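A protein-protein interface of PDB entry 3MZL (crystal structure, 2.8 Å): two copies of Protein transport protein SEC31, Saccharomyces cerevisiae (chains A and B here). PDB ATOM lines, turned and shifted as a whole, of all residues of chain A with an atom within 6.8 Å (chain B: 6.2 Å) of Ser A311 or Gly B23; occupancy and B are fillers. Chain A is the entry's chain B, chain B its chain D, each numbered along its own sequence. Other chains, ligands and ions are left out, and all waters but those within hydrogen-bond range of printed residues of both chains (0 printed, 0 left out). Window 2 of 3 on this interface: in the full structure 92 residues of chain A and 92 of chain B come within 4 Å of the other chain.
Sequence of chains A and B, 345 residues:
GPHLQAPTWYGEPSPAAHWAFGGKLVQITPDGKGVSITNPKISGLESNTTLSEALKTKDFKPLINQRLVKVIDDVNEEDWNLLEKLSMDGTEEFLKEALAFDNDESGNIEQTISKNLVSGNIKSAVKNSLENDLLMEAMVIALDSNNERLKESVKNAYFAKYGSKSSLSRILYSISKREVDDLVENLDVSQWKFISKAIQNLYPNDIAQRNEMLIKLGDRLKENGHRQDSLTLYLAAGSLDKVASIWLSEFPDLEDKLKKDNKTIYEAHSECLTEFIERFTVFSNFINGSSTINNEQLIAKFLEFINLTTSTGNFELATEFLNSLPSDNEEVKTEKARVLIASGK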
ATOM      1  N   TYR A 266      21.680  -1.777 -11.723  1.00  0.00           N
ATOM      2  CA  TYR A 266      21.961  -2.400 -13.016  1.00  0.00           C
ATOM      3  C   TYR A 266      20.701  -2.699 -13.827  1.00  0.00           C
ATOM      4  O   TYR A 266      20.642  -2.371 -15.013  1.00  0.00           O
ATOM      5  CB  TYR A 266      22.829  -3.657 -12.884  1.00  0.00           C
ATOM      6  CG  TYR A 266      23.071  -4.332 -14.219  1.00  0.00           C
ATOM      7  CD1 TYR A 266      23.879  -3.734 -15.187  1.00  0.00           C
ATOM      8  CD2 TYR A 266      22.471  -5.553 -14.524  1.00  0.00           C
ATOM      9  CE1 TYR A 266      24.092  -4.340 -16.419  1.00  0.00           C
ATOM     10  CE2 TYR A 266      22.679  -6.167 -15.756  1.00  0.00           C
ATOM     11  CZ  TYR A 266      23.490  -5.553 -16.697  1.00  0.00           C
ATOM     12  OH  TYR A 266      23.704  -6.156 -17.915  1.00  0.00           O
ATOM     13  N   ILE A 306      25.881  -1.657 -27.225  1.00  0.00           N
ATOM     14  CA  ILE A 306      26.761  -2.575 -27.962  1.00  0.00           C
ATOM     15  C   ILE A 306      27.489  -3.517 -26.999  1.00  0.00           C
ATOM     16  O   ILE A 306      27.570  -4.724 -27.245  1.00  0.00           O
ATOM     17  CB  ILE A 306      27.806  -1.814 -28.848  1.00  0.00           C
ATOM     18  CG1 ILE A 306      27.122  -0.897 -29.872  1.00  0.00           C
ATOM     19  CG2 ILE A 306      28.777  -2.785 -29.536  1.00  0.00           C
ATOM     20  CD1 ILE A 306      26.228  -1.606 -30.871  1.00  0.00           C
ATOM     21  N   ASN A 307      28.009  -2.952 -25.907  1.00  0.00           N
ATOM     22  CA  ASN A 307      28.686  -3.724 -24.866  1.00  0.00           C
ATOM     23  C   ASN A 307      27.729  -4.649 -24.110  1.00  0.00           C
ATOM     24  O   ASN A 307      28.132  -5.709 -23.629  1.00  0.00           O
ATOM     25  CB  ASN A 307      29.416  -2.796 -23.886  1.00  0.00           C
ATOM     26  CG  ASN A 307      30.446  -1.889 -24.572  1.00  0.00           C
ATOM     27  OD1 ASN A 307      30.918  -2.171 -25.679  1.00  0.00           O
ATOM     28  ND2 ASN A 307      30.802  -0.795 -23.903  1.00  0.00           N
ATOM     29  N   LEU A 308      26.462  -4.246 -24.017  1.00  0.00           N
ATOM     30  CA  LEU A 308      25.438  -5.056 -23.356  1.00  0.00           C
ATOM     31  C   LEU A 308      25.029  -6.261 -24.199  1.00  0.00           C
ATOM     32  O   LEU A 308      24.888  -7.367 -23.675  1.00  0.00           O
ATOM     33  CB  LEU A 308      24.197  -4.217 -23.013  1.00  0.00           C
ATOM     34  CG  LEU A 308      24.209  -3.174 -21.886  1.00  0.00           C
ATOM     35  CD1 LEU A 308      22.782  -2.769 -21.598  1.00  0.00           C
ATOM     36  CD2 LEU A 308      24.867  -3.675 -20.599  1.00  0.00           C
ATOM     37  N   THR A 309      24.843  -6.036 -25.498  1.00  0.00           N
ATOM     38  CA  THR A 309      24.409  -7.078 -26.433  1.00  0.00           C
ATOM     39  C   THR A 309      25.498  -8.132 -26.656  1.00  0.00           C
ATOM     40  O   THR A 309      25.209  -9.327 -26.710  1.00  0.00           O
ATOM     41  CB  THR A 309      23.955  -6.463 -27.783  1.00  0.00           C
ATOM     42  OG1 THR A 309      22.908  -5.519 -27.541  1.00  0.00           O
ATOM     43  CG2 THR A 309      23.438  -7.529 -28.735  1.00  0.00           C
ATOM     44  N   THR A 310      26.746  -7.683 -26.780  1.00  0.00           N
ATOM     45  CA  THR A 310      27.877  -8.600 -26.937  1.00  0.00           C
ATOM     46  C   THR A 310      28.086  -9.484 -25.707  1.00  0.00           C
ATOM     47  O   THR A 310      28.476 -10.643 -25.838  1.00  0.00           O
ATOM     48  CB  THR A 310      29.198  -7.865 -27.273  1.00  0.00           C
ATOM     49  OG1 THR A 310      29.356  -6.713 -26.432  1.00  0.00           O
ATOM     50  CG2 THR A 310      29.214  -7.431 -28.727  1.00  0.00           C
ATOM     51  N   SER A 311      27.819  -8.937 -24.522  1.00  0.00           N
ATOM     52  CA  SER A 311      28.002  -9.680 -23.278  1.00  0.00           C
ATOM     53  C   SER A 311      26.879 -10.696 -23.059  1.00  0.00           C
ATOM     54  O   SER A 311      26.926 -11.491 -22.116  1.00  0.00           O
ATOM     55  CB  SER A 311      28.110  -8.733 -22.082  1.00  0.00           C
ATOM     56  OG  SER A 311      26.834  -8.484 -21.518  1.00  0.00           O
ATOM     57  N   THR A 312      25.868 -10.653 -23.924  1.00  0.00           N
ATOM     58  CA  THR A 312      24.822 -11.668 -23.931  1.00  0.00           C
ATOM     59  C   THR A 312      25.214 -12.822 -24.853  1.00  0.00           C
ATOM     60  O   THR A 312      24.641 -13.911 -24.769  1.00  0.00           O
ATOM     61  CB  THR A 312      23.436 -11.094 -24.352  1.00  0.00           C
ATOM     62  OG1 THR A 312      23.461 -10.689 -25.727  1.00  0.00           O
ATOM     63  CG2 THR A 312      23.052  -9.903 -23.484  1.00  0.00           C
ATOM     64  N   GLY A 313      26.192 -12.575 -25.726  1.00  0.00           N
ATOM     65  CA  GLY A 313      26.680 -13.575 -26.681  1.00  0.00           C
ATOM     66  C   GLY A 313      26.212 -13.339 -28.107  1.00  0.00           C
ATOM     67  O   GLY A 313      26.722 -13.954 -29.049  1.00  0.00           O
ATOM     68  N   ASN A 314      25.243 -12.434 -28.254  1.00  0.00           N
ATOM     69  CA  ASN A 314      24.598 -12.130 -29.530  1.00  0.00           C
ATOM     70  C   ASN A 314      25.395 -11.113 -30.361  1.00  0.00           C
ATOM     71  O   ASN A 314      25.093  -9.916 -30.362  1.00  0.00           O
ATOM     72  CB  ASN A 314      23.172 -11.632 -29.258  1.00  0.00           C
ATOM     73  CG  ASN A 314      22.350 -11.429 -30.524  1.00  0.00           C
ATOM     74  OD1 ASN A 314      22.823 -11.624 -31.644  1.00  0.00           O
ATOM     75  ND2 ASN A 314      21.099 -11.024 -30.342  1.00  0.00           N
ATOM     76  N   PHE A 315      26.410 -11.602 -31.073  1.00  0.00           N
ATOM     77  CA  PHE A 315      27.274 -10.748 -31.896  1.00  0.00           C
ATOM     78  C   PHE A 315      26.578 -10.246 -33.162  1.00  0.00           C
ATOM     79  O   PHE A 315      26.881  -9.160 -33.663  1.00  0.00           O
ATOM     80  CB  PHE A 315      28.564 -11.488 -32.267  1.00  0.00           C
ATOM     81  CG  PHE A 315      29.375 -11.929 -31.080  1.00  0.00           C
ATOM     82  CD1 PHE A 315      29.561 -13.284 -30.814  1.00  0.00           C
ATOM     83  CD2 PHE A 315      29.952 -10.995 -30.225  1.00  0.00           C
ATOM     84  CE1 PHE A 315      30.314 -13.701 -29.720  1.00  0.00           C
ATOM     85  CE2 PHE A 315      30.697 -11.403 -29.127  1.00  0.00           C
ATOM     86  CZ  PHE A 315      30.880 -12.759 -28.877  1.00  0.00           C
ATOM     87  N   TRP B  19      35.713 -14.916 -16.643  1.00  0.00           N
ATOM     88  CA  TRP B  19      34.747 -14.466 -17.638  1.00  0.00           C
ATOM     89  C   TRP B  19      35.517 -13.985 -18.853  1.00  0.00           C
ATOM     90  O   TRP B  19      36.614 -13.435 -18.715  1.00  0.00           O
ATOM     91  CB  TRP B  19      33.895 -13.313 -17.106  1.00  0.00           C
ATOM     92  CG  TRP B  19      32.857 -13.719 -16.126  1.00  0.00           C
ATOM     93  CD1 TRP B  19      32.886 -13.526 -14.779  1.00  0.00           C
ATOM     94  CD2 TRP B  19      31.624 -14.387 -16.410  1.00  0.00           C
ATOM     95  NE1 TRP B  19      31.746 -14.026 -14.202  1.00  0.00           N
ATOM     96  CE2 TRP B  19      30.953 -14.563 -15.181  1.00  0.00           C
ATOM     97  CE3 TRP B  19      31.019 -14.850 -17.585  1.00  0.00           C
ATOM     98  CZ2 TRP B  19      29.707 -15.187 -15.090  1.00  0.00           C
ATOM     99  CZ3 TRP B  19      29.778 -15.468 -17.494  1.00  0.00           C
ATOM    100  CH2 TRP B  19      29.139 -15.635 -16.252  1.00  0.00           C
ATOM    101  N   ALA B  20      34.935 -14.188 -20.031  1.00  0.00           N
ATOM    102  CA  ALA B  20      35.535 -13.762 -21.288  1.00  0.00           C
ATOM    103  C   ALA B  20      34.481 -13.161 -22.206  1.00  0.00           C
ATOM    104  O   ALA B  20      33.288 -13.469 -22.074  1.00  0.00           O
ATOM    105  CB  ALA B  20      36.226 -14.927 -21.965  1.00  0.00           C
ATOM    106  N   PHE B  21      34.940 -12.318 -23.136  1.00  0.00           N
ATOM    107  CA  PHE B  21      34.084 -11.578 -24.065  1.00  0.00           C
ATOM    108  C   PHE B  21      33.075 -12.447 -24.798  1.00  0.00           C
ATOM    109  O   PHE B  21      33.447 -13.333 -25.569  1.00  0.00           O
ATOM    110  CB  PHE B  21      34.936 -10.796 -25.070  1.00  0.00           C
ATOM    111  CG  PHE B  21      34.133  -9.916 -26.007  1.00  0.00           C
ATOM    112  CD1 PHE B  21      33.528  -8.748 -25.543  1.00  0.00           C
ATOM    113  CD2 PHE B  21      33.995 -10.250 -27.352  1.00  0.00           C
ATOM    114  CE1 PHE B  21      32.798  -7.934 -26.402  1.00  0.00           C
ATOM    115  CE2 PHE B  21      33.267  -9.440 -28.218  1.00  0.00           C
ATOM    116  CZ  PHE B  21      32.671  -8.280 -27.745  1.00  0.00           C
ATOM    117  N   GLY B  22      31.795 -12.183 -24.544  1.00  0.00           N
ATOM    118  CA  GLY B  22      30.697 -12.889 -25.206  1.00  0.00           C
ATOM    119  C   GLY B  22      29.924 -13.845 -24.313  1.00  0.00           C
ATOM    120  O   GLY B  22      29.342 -14.818 -24.797  1.00  0.00           O
ATOM    121  N   GLY B  23      29.918 -13.564 -23.013  1.00  0.00           N
ATOM    122  CA  GLY B  23      29.218 -14.400 -22.040  1.00  0.00           C
ATOM    123  C   GLY B  23      29.893 -15.734 -21.771  1.00  0.00           C
ATOM    124  O   GLY B  23      29.305 -16.618 -21.149  1.00  0.00           O
ATOM    125  N   LYS B  24      31.130 -15.879 -22.237  1.00  0.00           N
ATOM    126  CA  LYS B  24      31.882 -17.120 -22.052  1.00  0.00           C
ATOM    127  C   LYS B  24      32.431 -17.225 -20.635  1.00  0.00           C
ATOM    128  O   LYS B  24      32.834 -16.228 -20.037  1.00  0.00           O
ATOM    129  CB  LYS B  24      33.028 -17.237 -23.072  1.00  0.00           C
ATOM    130  CG  LYS B  24      32.575 -17.351 -24.526  1.00  0.00           C
ATOM    131  CD  LYS B  24      33.732 -17.673 -25.460  1.00  0.00           C
ATOM    132  CE  LYS B  24      33.250 -18.293 -26.764  1.00  0.00           C
ATOM    133  NZ  LYS B  24      32.583 -17.309 -27.664  1.00  0.00           N
ATOM    134  N   LEU B  25      32.421 -18.443 -20.106  1.00  0.00           N
ATOM    135  CA  LEU B  25      33.076 -18.739 -18.841  1.00  0.00           C
ATOM    136  C   LEU B  25      34.084 -19.869 -19.026  1.00  0.00           C
ATOM    137  O   LEU B  25      33.712 -21.010 -19.314  1.00  0.00           O
ATOM    138  CB  LEU B  25      32.065 -19.072 -17.735  1.00  0.00           C
ATOM    139  CG  LEU B  25      32.638 -19.291 -16.325  1.00  0.00           C
ATOM    140  CD1 LEU B  25      33.330 -18.042 -15.781  1.00  0.00           C
ATOM    141  CD2 LEU B  25      31.561 -19.772 -15.360  1.00  0.00           C
ATOM    142  N   THR B  38      32.291 -22.576 -21.528  1.00  0.00           N
ATOM    143  CA  THR B  38      30.836 -22.616 -21.723  1.00  0.00           C
ATOM    144  C   THR B  38      30.225 -21.214 -21.796  1.00  0.00           C
ATOM    145  O   THR B  38      30.893 -20.225 -21.488  1.00  0.00           O
ATOM    146  CB  THR B  38      30.130 -23.403 -20.602  1.00  0.00           C
ATOM    147  OG1 THR B  38      30.261 -22.697 -19.364  1.00  0.00           O
ATOM    148  CG2 THR B  38      30.725 -24.798 -20.456  1.00  0.00           C
ATOM    149  N   ASN B  39      28.960 -21.142 -22.214  1.00  0.00           N
ATOM    150  CA  ASN B  39      28.204 -19.892 -22.222  1.00  0.00           C
ATOM    151  C   ASN B  39      27.054 -19.947 -21.216  1.00  0.00           C
ATOM    152  O   ASN B  39      25.930 -20.305 -21.580  1.00  0.00           O
ATOM    153  CB  ASN B  39      27.672 -19.586 -23.626  1.00  0.00           C
ATOM    154  CG  ASN B  39      28.753 -19.084 -24.568  1.00  0.00           C
ATOM    155  OD1 ASN B  39      29.257 -19.831 -25.407  1.00  0.00           O
ATOM    156  ND2 ASN B  39      29.117 -17.814 -24.430  1.00  0.00           N
ATOM    157  N   PRO B  40      27.330 -19.604 -19.941  1.00  0.00           N
ATOM    158  CA  PRO B  40      26.289 -19.692 -18.916  1.00  0.00           C
ATOM    159  C   PRO B  40      25.095 -18.794 -19.220  1.00  0.00           C
ATOM    160  O   PRO B  40      25.266 -17.607 -19.526  1.00  0.00           O
ATOM    161  CB  PRO B  40      26.999 -19.216 -17.645  1.00  0.00           C
ATOM    162  CG  PRO B  40      28.443 -19.427 -17.915  1.00  0.00           C
ATOM    163  CD  PRO B  40      28.613 -19.153 -19.372  1.00  0.00           C
ATOM    164  N   LEU B  45      19.579 -11.779 -17.650  1.00  0.00           N
ATOM    165  CA  LEU B  45      20.332 -11.356 -18.827  1.00  0.00           C
ATOM    166  C   LEU B  45      20.155 -12.380 -19.948  1.00  0.00           C
ATOM    167  O   LEU B  45      20.543 -13.544 -19.812  1.00  0.00           O
ATOM    168  CB  LEU B  45      21.807 -11.153 -18.460  1.00  0.00           C
ATOM    169  CG  LEU B  45      22.737 -10.474 -19.468  1.00  0.00           C
ATOM    170  CD1 LEU B  45      23.543  -9.370 -18.803  1.00  0.00           C
ATOM    171  CD2 LEU B  45      23.651 -11.496 -20.129  1.00  0.00           C
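No position is printed for both chains.
Of the 9 pairs that touch across the chains among the printed residues, none has its exchanged pair printed and touching as well.
Of the printed residues of chain B, Thr A310 touches Phe B21 and Gly B22.
Ser A311 touches just these residues of chain B: Gly B23 and Leu B45.
Of the printed residues of chain B, Thr A312 touches Leu B45.
Of the printed residues of chain A, Phe B21 touches Thr A310 (3.5 Å) and Phe A315 (3.4 Å).
Printed residues of chain A within 4 Å of Gly B23: Ser A311.
The nearest printed residue of chain A that does not touch Gly B22 is Ser A311 (4.4 Å).
Printed residues of chain A that touch a printed residue of chain B: Tyr A266, Thr A310, Ser A311, Thr A312, Gly A313 and Phe A315.
Of the 11 printed residues of chain B, 4 touch a printed residue of chain A.
Hydrophobic or aromatic side chains of chain B that line the printed part of chain A: Phe B21 and Leu B45.
Among the printed residues, 9 pairs touch across the chains.
Among the printed residues, no Asp or Glu carboxylate lies within 4 Å of a Lys or Arg side-chain nitrogen of the other chain.
OG1 of Thr A310 sits at hydrogen-bond distance from O of Ile A306 (2.8 Å).
The backbone carbonyl oxygen (O) of Asn A307 sits at hydrogen-bond distance from the side-chain hydroxyl (OG1) of Thr A310, at 3.2 Å.
O of Leu A308 lies within hydrogen-bond range of OG of Ser A311, at 3.1 Å.
O of Thr A309 lies within hydrogen-bond range of OG1 of Thr A312, 2.4 Å away.
ND2 of Asn B39 sits at hydrogen-bond distance from O of Gly B22, at 3.0 Å.
The backbone carbonyl oxygen (O) of Gly B23 sits close to the side-chain amide nitrogen (ND2) of Asn B39, at 3.5 Å.
Among the printed residues, merely in contact across the chains: Tyr A266 with Leu B45 (3.3 Å), Thr A310 with Phe B21 (3.5 Å), Thr A310 with Gly B22 (3.2 Å), Ser A311 with Gly B23 (3.7 Å), Ser A311 with Leu B45 (3.8 Å), Thr A312 with Leu B45 (3.8 Å), Gly A313 with Gly B22 (3.5 Å), Phe A315 with Phe B21 (3.4 Å) and Phe A315 with Gly B22 (3.7 Å).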
